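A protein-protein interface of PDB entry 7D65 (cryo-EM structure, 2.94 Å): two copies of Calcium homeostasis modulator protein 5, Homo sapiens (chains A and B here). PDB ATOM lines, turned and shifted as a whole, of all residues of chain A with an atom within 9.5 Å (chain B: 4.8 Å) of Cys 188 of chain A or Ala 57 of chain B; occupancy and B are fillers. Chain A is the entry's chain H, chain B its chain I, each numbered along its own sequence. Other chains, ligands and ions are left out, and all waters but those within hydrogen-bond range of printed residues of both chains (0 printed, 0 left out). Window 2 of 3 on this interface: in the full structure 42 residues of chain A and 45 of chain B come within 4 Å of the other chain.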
ATOM      1  N   VAL A 112      -8.197  -7.424 -17.443  1.00  0.00           N
ATOM      2  CA  VAL A 112      -7.643  -8.072 -18.625  1.00  0.00           C
ATOM      3  C   VAL A 112      -7.705  -9.587 -18.481  1.00  0.00           C
ATOM      4  O   VAL A 112      -7.920 -10.305 -19.462  1.00  0.00           O
ATOM      5  CB  VAL A 112      -6.223  -7.527 -18.874  1.00  0.00           C
ATOM      6  CG1 VAL A 112      -5.463  -8.334 -19.893  1.00  0.00           C
ATOM      7  CG2 VAL A 112      -6.321  -6.108 -19.364  1.00  0.00           C
ATOM      8  N   SER A 116     -10.050 -12.094 -21.241  1.00  0.00           N
ATOM      9  CA  SER A 116      -9.350 -13.165 -21.931  1.00  0.00           C
ATOM     10  C   SER A 116     -10.034 -14.507 -21.727  1.00  0.00           C
ATOM     11  O   SER A 116     -10.166 -15.284 -22.673  1.00  0.00           O
ATOM     12  CB  SER A 116      -7.907 -13.233 -21.453  1.00  0.00           C
ATOM     13  OG  SER A 116      -7.334 -11.943 -21.439  1.00  0.00           O
ATOM     14  N   LEU A 120     -12.283 -16.728 -24.582  1.00  0.00           N
ATOM     15  CA  LEU A 120     -11.823 -18.071 -24.899  1.00  0.00           C
ATOM     16  C   LEU A 120     -12.910 -19.112 -24.705  1.00  0.00           C
ATOM     17  O   LEU A 120     -12.839 -20.184 -25.305  1.00  0.00           O
ATOM     18  CB  LEU A 120     -10.618 -18.439 -24.040  1.00  0.00           C
ATOM     19  CG  LEU A 120      -9.239 -17.946 -24.467  1.00  0.00           C
ATOM     20  CD1 LEU A 120      -8.195 -18.425 -23.488  1.00  0.00           C
ATOM     21  CD2 LEU A 120      -8.906 -18.434 -25.840  1.00  0.00           C
ATOM     22  N   GLN A 180     -12.023 -17.065 -29.979  1.00  0.00           N
ATOM     23  CA  GLN A 180     -10.854 -17.710 -29.406  1.00  0.00           C
ATOM     24  C   GLN A 180      -9.568 -17.250 -30.065  1.00  0.00           C
ATOM     25  O   GLN A 180      -8.502 -17.410 -29.476  1.00  0.00           O
ATOM     26  CB  GLN A 180     -10.989 -19.220 -29.503  1.00  0.00           C
ATOM     27  CG  GLN A 180     -11.999 -19.772 -28.551  1.00  0.00           C
ATOM     28  CD  GLN A 180     -12.111 -21.258 -28.625  1.00  0.00           C
ATOM     29  OE1 GLN A 180     -12.146 -21.832 -29.702  1.00  0.00           O
ATOM     30  NE2 GLN A 180     -12.170 -21.900 -27.475  1.00  0.00           N
ATOM     31  N   ILE A 181      -9.638 -16.680 -31.263  1.00  0.00           N
ATOM     32  CA  ILE A 181      -8.465 -16.038 -31.837  1.00  0.00           C
ATOM     33  C   ILE A 181      -8.236 -14.675 -31.192  1.00  0.00           C
ATOM     34  O   ILE A 181      -7.105 -14.329 -30.841  1.00  0.00           O
ATOM     35  CB  ILE A 181      -8.612 -15.954 -33.365  1.00  0.00           C
ATOM     36  CG1 ILE A 181      -8.308 -17.308 -33.985  1.00  0.00           C
ATOM     37  CG2 ILE A 181      -7.697 -14.922 -33.964  1.00  0.00           C
ATOM     38  CD1 ILE A 181      -8.674 -17.396 -35.418  1.00  0.00           C
ATOM     39  N   LEU A 182      -9.302 -13.895 -30.983  1.00  0.00           N
ATOM     40  CA  LEU A 182      -9.193 -12.630 -30.257  1.00  0.00           C
ATOM     41  C   LEU A 182      -8.893 -12.821 -28.782  1.00  0.00           C
ATOM     42  O   LEU A 182      -8.402 -11.891 -28.144  1.00  0.00           O
ATOM     43  CB  LEU A 182     -10.478 -11.820 -30.372  1.00  0.00           C
ATOM     44  CG  LEU A 182     -10.884 -11.322 -31.744  1.00  0.00           C
ATOM     45  CD1 LEU A 182     -12.075 -10.421 -31.606  1.00  0.00           C
ATOM     46  CD2 LEU A 182      -9.739 -10.600 -32.392  1.00  0.00           C
ATOM     47  N   GLY A 183      -9.213 -13.980 -28.218  1.00  0.00           N
ATOM     48  CA  GLY A 183      -8.825 -14.251 -26.850  1.00  0.00           C
ATOM     49  C   GLY A 183      -7.326 -14.371 -26.693  1.00  0.00           C
ATOM     50  O   GLY A 183      -6.764 -13.903 -25.706  1.00  0.00           O
ATOM     51  N   TRP A 184      -6.652 -14.976 -27.673  1.00  0.00           N
ATOM     52  CA  TRP A 184      -5.207 -15.154 -27.609  1.00  0.00           C
ATOM     53  C   TRP A 184      -4.436 -13.927 -28.057  1.00  0.00           C
ATOM     54  O   TRP A 184      -3.280 -13.772 -27.667  1.00  0.00           O
ATOM     55  CB  TRP A 184      -4.766 -16.341 -28.460  1.00  0.00           C
ATOM     56  CG  TRP A 184      -5.056 -17.671 -27.865  1.00  0.00           C
ATOM     57  CD1 TRP A 184      -5.897 -18.607 -28.357  1.00  0.00           C
ATOM     58  CD2 TRP A 184      -4.495 -18.227 -26.673  1.00  0.00           C
ATOM     59  NE1 TRP A 184      -5.916 -19.707 -27.548  1.00  0.00           N
ATOM     60  CE2 TRP A 184      -5.057 -19.500 -26.506  1.00  0.00           C
ATOM     61  CE3 TRP A 184      -3.577 -17.770 -25.727  1.00  0.00           C
ATOM     62  CZ2 TRP A 184      -4.735 -20.319 -25.437  1.00  0.00           C
ATOM     63  CZ3 TRP A 184      -3.262 -18.582 -24.669  1.00  0.00           C
ATOM     64  CH2 TRP A 184      -3.839 -19.841 -24.530  1.00  0.00           C
ATOM     65  N   CYS A 185      -5.035 -13.057 -28.868  1.00  0.00           N
ATOM     66  CA  CYS A 185      -4.365 -11.820 -29.246  1.00  0.00           C
ATOM     67  C   CYS A 185      -4.326 -10.818 -28.104  1.00  0.00           C
ATOM     68  O   CYS A 185      -3.544  -9.868 -28.156  1.00  0.00           O
ATOM     69  CB  CYS A 185      -5.052 -11.190 -30.452  1.00  0.00           C
ATOM     70  SG  CYS A 185      -4.511 -11.835 -32.037  1.00  0.00           S
ATOM     71  N   LEU A 186      -5.152 -11.009 -27.085  1.00  0.00           N
ATOM     72  CA  LEU A 186      -5.189 -10.135 -25.926  1.00  0.00           C
ATOM     73  C   LEU A 186      -4.261 -10.597 -24.816  1.00  0.00           C
ATOM     74  O   LEU A 186      -3.714  -9.760 -24.098  1.00  0.00           O
ATOM     75  CB  LEU A 186      -6.621 -10.039 -25.401  1.00  0.00           C
ATOM     76  CG  LEU A 186      -6.961  -9.010 -24.333  1.00  0.00           C
ATOM     77  CD1 LEU A 186      -7.164  -7.656 -24.954  1.00  0.00           C
ATOM     78  CD2 LEU A 186      -8.200  -9.454 -23.613  1.00  0.00           C
ATOM     79  N   ILE A 187      -4.071 -11.906 -24.644  1.00  0.00           N
ATOM     80  CA  ILE A 187      -3.080 -12.363 -23.678  1.00  0.00           C
ATOM     81  C   ILE A 187      -1.677 -12.119 -24.203  1.00  0.00           C
ATOM     82  O   ILE A 187      -0.750 -11.878 -23.427  1.00  0.00           O
ATOM     83  CB  ILE A 187      -3.284 -13.847 -23.332  1.00  0.00           C
ATOM     84  CG1 ILE A 187      -4.761 -14.157 -23.183  1.00  0.00           C
ATOM     85  CG2 ILE A 187      -2.599 -14.188 -22.034  1.00  0.00           C
ATOM     86  CD1 ILE A 187      -5.057 -15.600 -22.887  1.00  0.00           C
ATOM     87  N   CYS A 188      -1.494 -12.157 -25.518  1.00  0.00           N
ATOM     88  CA  CYS A 188      -0.159 -12.046 -26.083  1.00  0.00           C
ATOM     89  C   CYS A 188       0.318 -10.607 -26.160  1.00  0.00           C
ATOM     90  O   CYS A 188       1.522 -10.359 -26.073  1.00  0.00           O
ATOM     91  CB  CYS A 188      -0.121 -12.685 -27.467  1.00  0.00           C
ATOM     92  SG  CYS A 188      -0.083 -14.472 -27.425  1.00  0.00           S
ATOM     93  N   SER A 189      -0.583  -9.649 -26.335  1.00  0.00           N
ATOM     94  CA  SER A 189      -0.167  -8.260 -26.421  1.00  0.00           C
ATOM     95  C   SER A 189      -0.171  -7.560 -25.077  1.00  0.00           C
ATOM     96  O   SER A 189       0.498  -6.536 -24.928  1.00  0.00           O
ATOM     97  CB  SER A 189      -1.057  -7.493 -27.395  1.00  0.00           C
ATOM     98  OG  SER A 189      -2.331  -7.263 -26.834  1.00  0.00           O
ATOM     99  N   ALA A 190      -0.907  -8.079 -24.097  1.00  0.00           N
ATOM    100  CA  ALA A 190      -0.828  -7.529 -22.753  1.00  0.00           C
ATOM    101  C   ALA A 190       0.381  -8.054 -22.002  1.00  0.00           C
ATOM    102  O   ALA A 190       0.939  -7.333 -21.175  1.00  0.00           O
ATOM    103  CB  ALA A 190      -2.094  -7.843 -21.964  1.00  0.00           C
ATOM    104  N   SER A 191       0.791  -9.295 -22.262  1.00  0.00           N
ATOM    105  CA  SER A 191       2.000  -9.817 -21.638  1.00  0.00           C
ATOM    106  C   SER A 191       3.249  -9.160 -22.201  1.00  0.00           C
ATOM    107  O   SER A 191       4.216  -8.944 -21.468  1.00  0.00           O
ATOM    108  CB  SER A 191       2.077 -11.329 -21.820  1.00  0.00           C
ATOM    109  OG  SER A 191       1.267 -11.992 -20.869  1.00  0.00           O
ATOM    110  N   PHE A 192       3.245  -8.829 -23.488  1.00  0.00           N
ATOM    111  CA  PHE A 192       4.369  -8.116 -24.072  1.00  0.00           C
ATOM    112  C   PHE A 192       4.416  -6.663 -23.616  1.00  0.00           C
ATOM    113  O   PHE A 192       5.501  -6.099 -23.470  1.00  0.00           O
ATOM    114  CB  PHE A 192       4.289  -8.195 -25.590  1.00  0.00           C
ATOM    115  CG  PHE A 192       5.382  -7.466 -26.291  1.00  0.00           C
ATOM    116  CD1 PHE A 192       6.690  -7.894 -26.186  1.00  0.00           C
ATOM    117  CD2 PHE A 192       5.102  -6.357 -27.063  1.00  0.00           C
ATOM    118  CE1 PHE A 192       7.700  -7.228 -26.835  1.00  0.00           C
ATOM    119  CE2 PHE A 192       6.107  -5.687 -27.716  1.00  0.00           C
ATOM    120  CZ  PHE A 192       7.407  -6.122 -27.602  1.00  0.00           C
ATOM    121  N   PHE A 193       3.260  -6.042 -23.389  1.00  0.00           N
ATOM    122  CA  PHE A 193       3.229  -4.669 -22.898  1.00  0.00           C
ATOM    123  C   PHE A 193       3.586  -4.588 -21.423  1.00  0.00           C
ATOM    124  O   PHE A 193       4.210  -3.616 -20.994  1.00  0.00           O
ATOM    125  CB  PHE A 193       1.847  -4.062 -23.145  1.00  0.00           C
ATOM    126  CG  PHE A 193       1.679  -2.667 -22.612  1.00  0.00           C
ATOM    127  CD1 PHE A 193       2.204  -1.585 -23.293  1.00  0.00           C
ATOM    128  CD2 PHE A 193       0.966  -2.436 -21.443  1.00  0.00           C
ATOM    129  CE1 PHE A 193       2.042  -0.297 -22.807  1.00  0.00           C
ATOM    130  CE2 PHE A 193       0.805  -1.154 -20.950  1.00  0.00           C
ATOM    131  CZ  PHE A 193       1.340  -0.085 -21.635  1.00  0.00           C
ATOM    132  N   SER A 194       3.195  -5.588 -20.636  1.00  0.00           N
ATOM    133  CA  SER A 194       3.522  -5.610 -19.217  1.00  0.00           C
ATOM    134  C   SER A 194       5.002  -5.849 -18.959  1.00  0.00           C
ATOM    135  O   SER A 194       5.491  -5.498 -17.883  1.00  0.00           O
ATOM    136  CB  SER A 194       2.701  -6.680 -18.510  1.00  0.00           C
ATOM    137  OG  SER A 194       3.350  -7.124 -17.340  1.00  0.00           O
ATOM    138  N   LEU A 195       5.723  -6.449 -19.903  1.00  0.00           N
ATOM    139  CA  LEU A 195       7.163  -6.603 -19.748  1.00  0.00           C
ATOM    140  C   LEU A 195       7.912  -5.359 -20.187  1.00  0.00           C
ATOM    141  O   LEU A 195       8.962  -5.046 -19.626  1.00  0.00           O
ATOM    142  CB  LEU A 195       7.650  -7.813 -20.544  1.00  0.00           C
ATOM    143  CG  LEU A 195       9.111  -8.241 -20.403  1.00  0.00           C
ATOM    144  CD1 LEU A 195       9.334  -9.008 -19.119  1.00  0.00           C
ATOM    145  CD2 LEU A 195       9.535  -9.061 -21.599  1.00  0.00           C
ATOM    146  N   VAL B  53      -2.534 -20.712 -34.000  1.00  0.00           N
ATOM    147  CA  VAL B  53      -2.537 -19.835 -32.834  1.00  0.00           C
ATOM    148  C   VAL B  53      -2.563 -20.647 -31.547  1.00  0.00           C
ATOM    149  O   VAL B  53      -1.870 -20.322 -30.586  1.00  0.00           O
ATOM    150  CB  VAL B  53      -3.722 -18.851 -32.940  1.00  0.00           C
ATOM    151  CG1 VAL B  53      -4.132 -18.284 -31.607  1.00  0.00           C
ATOM    152  CG2 VAL B  53      -3.364 -17.717 -33.862  1.00  0.00           C
ATOM    153  N   LEU B  55      -1.065 -23.357 -31.294  1.00  0.00           N
ATOM    154  CA  LEU B  55       0.237 -23.995 -31.284  1.00  0.00           C
ATOM    155  C   LEU B  55       1.325 -23.040 -30.818  1.00  0.00           C
ATOM    156  O   LEU B  55       2.160 -23.412 -29.991  1.00  0.00           O
ATOM    157  CB  LEU B  55       0.538 -24.520 -32.688  1.00  0.00           C
ATOM    158  CG  LEU B  55       1.659 -25.482 -33.020  1.00  0.00           C
ATOM    159  CD1 LEU B  55       1.427 -26.783 -32.309  1.00  0.00           C
ATOM    160  CD2 LEU B  55       1.649 -25.687 -34.507  1.00  0.00           C
ATOM    161  N   PHE B  56       1.308 -21.801 -31.305  1.00  0.00           N
ATOM    162  CA  PHE B  56       2.391 -20.853 -31.084  1.00  0.00           C
ATOM    163  C   PHE B  56       2.128 -19.834 -29.987  1.00  0.00           C
ATOM    164  O   PHE B  56       3.079 -19.394 -29.339  1.00  0.00           O
ATOM    165  CB  PHE B  56       2.699 -20.099 -32.375  1.00  0.00           C
ATOM    166  CG  PHE B  56       3.430 -20.913 -33.392  1.00  0.00           C
ATOM    167  CD1 PHE B  56       4.455 -21.755 -33.016  1.00  0.00           C
ATOM    168  CD2 PHE B  56       3.100 -20.829 -34.728  1.00  0.00           C
ATOM    169  CE1 PHE B  56       5.130 -22.500 -33.955  1.00  0.00           C
ATOM    170  CE2 PHE B  56       3.773 -21.571 -35.667  1.00  0.00           C
ATOM    171  CZ  PHE B  56       4.786 -22.406 -35.277  1.00  0.00           C
ATOM    172  N   ALA B  57       0.889 -19.423 -29.762  1.00  0.00           N
ATOM    173  CA  ALA B  57       0.630 -18.378 -28.773  1.00  0.00           C
ATOM    174  C   ALA B  57       0.783 -18.797 -27.308  1.00  0.00           C
ATOM    175  O   ALA B  57       1.145 -17.939 -26.500  1.00  0.00           O
ATOM    176  CB  ALA B  57      -0.752 -17.760 -28.985  1.00  0.00           C
ATOM    177  N   PRO B  58       0.516 -20.040 -26.878  1.00  0.00           N
ATOM    178  CA  PRO B  58       0.963 -20.418 -25.530  1.00  0.00           C
ATOM    179  C   PRO B  58       2.462 -20.623 -25.404  1.00  0.00           C
ATOM    180  O   PRO B  58       2.944 -20.789 -24.281  1.00  0.00           O
ATOM    181  CB  PRO B  58       0.203 -21.717 -25.261  1.00  0.00           C
ATOM    182  CG  PRO B  58      -0.982 -21.600 -26.065  1.00  0.00           C
ATOM    183  CD  PRO B  58      -0.518 -20.989 -27.328  1.00  0.00           C
ATOM    184  N   ALA B  59       3.212 -20.630 -26.502  1.00  0.00           N
ATOM    185  CA  ALA B  59       4.663 -20.672 -26.438  1.00  0.00           C
ATOM    186  C   ALA B  59       5.271 -19.286 -26.335  1.00  0.00           C
ATOM    187  O   ALA B  59       6.375 -19.143 -25.808  1.00  0.00           O
ATOM    188  CB  ALA B  59       5.228 -21.387 -27.664  1.00  0.00           C
ATOM    189  N   TRP B  60       4.578 -18.266 -26.830  1.00  0.00           N
ATOM    190  CA  TRP B  60       5.030 -16.890 -26.687  1.00  0.00           C
ATOM    191  C   TRP B  60       4.763 -16.353 -25.290  1.00  0.00           C
ATOM    192  O   TRP B  60       5.506 -15.498 -24.807  1.00  0.00           O
ATOM    193  CB  TRP B  60       4.347 -16.028 -27.747  1.00  0.00           C
ATOM    194  CG  TRP B  60       4.435 -14.557 -27.553  1.00  0.00           C
ATOM    195  CD1 TRP B  60       3.533 -13.759 -26.919  1.00  0.00           C
ATOM    196  CD2 TRP B  60       5.468 -13.694 -28.028  1.00  0.00           C
ATOM    197  NE1 TRP B  60       3.947 -12.456 -26.953  1.00  0.00           N
ATOM    198  CE2 TRP B  60       5.132 -12.389 -27.634  1.00  0.00           C
ATOM    199  CE3 TRP B  60       6.650 -13.899 -28.740  1.00  0.00           C
ATOM    200  CZ2 TRP B  60       5.933 -11.295 -27.927  1.00  0.00           C
ATOM    201  CZ3 TRP B  60       7.442 -12.810 -29.032  1.00  0.00           C
ATOM    202  CH2 TRP B  60       7.083 -11.525 -28.626  1.00  0.00           C
ATOM    203  N   VAL B  61       3.717 -16.836 -24.628  1.00  0.00           N
ATOM    204  CA  VAL B  61       3.432 -16.405 -23.264  1.00  0.00           C
ATOM    205  C   VAL B  61       4.404 -17.059 -22.291  1.00  0.00           C
ATOM    206  O   VAL B  61       4.893 -16.416 -21.356  1.00  0.00           O
ATOM    207  CB  VAL B  61       1.959 -16.709 -22.927  1.00  0.00           C
ATOM    208  CG1 VAL B  61       1.690 -16.667 -21.440  1.00  0.00           C
ATOM    209  CG2 VAL B  61       1.056 -15.735 -23.640  1.00  0.00           C
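The side-chain sulfur (SG) of Cys 188 of chain A sits close to the backbone carbonyl oxygen (O) of Ala 57 of chain B, at 3.8 Å. The backbone carbonyl oxygen (O) of Cys 188 of chain A is in hydrogen-bond range of the indole nitrogen (NE1) of Trp 60 of chain B (3.3 Å).
SG of Cys 188 of chain A lies within hydrogen-bond range of O of Trp 184 of chain A (3.3 Å).
CD1 of Trp 184 of chain A touches CG1 of Val 53 of chain B, 3.7 Å away. Trp 184 of chain A touches Pro 58 of chain B. Phe 192 of chain A touches Trp 60 of chain B (CD1 to CZ2, 3.9 Å).
Ser 116 of chain A touches none of the printed residues of chain B. Of the printed residues of chain B, Trp 184 of chain A touches Val 53 (3.7 Å) and Pro 58 (3.7 Å). Printed residues of chain B within 4 Å of Cys 188 of chain A: Ala 57 and Trp 60. Of the printed residues of chain A, Val 53 of chain B touches Trp 184. Ala 57 of chain B touches one residue of chain A. Pro 58 of chain B touches just one residue of chain A: Trp 184. No residue of chain A comes within 4 Å of Ala 59 of chain B. Of the printed residues of chain A, Trp 60 of chain B touches Cys 188 (3.3 Å) and Phe 192 (3.9 Å). The nearest printed residue of chain A that does not touch Val 53 of chain B is Ile 181 of chain A (4.9 Å).
Printed residues of chain B that touch a printed residue of chain A: Val 53, Ala 57, Pro 58 and Trp 60. Hydrophobic or aromatic side chains of chain B within 4 Å of the printed part of chain A: Val 53, Ala 57, Pro 58 and Trp 60. Of the 19 printed residues of chain A, 3 touch a printed residue of chain B. Printed residues of chain A that touch a printed residue of chain B: Trp 184, Cys 188 and Phe 192. Among the printed residues, 5 pairs touch across the chains. Among the printed residues, no Asp or Glu carboxylate lies within 4 Å of a Lys or Arg side-chain nitrogen of the other chain.
No position is printed for both chains. Of the 5 pairs that touch across the chains among the printed residues, none has its exchanged pair printed and touching as well.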
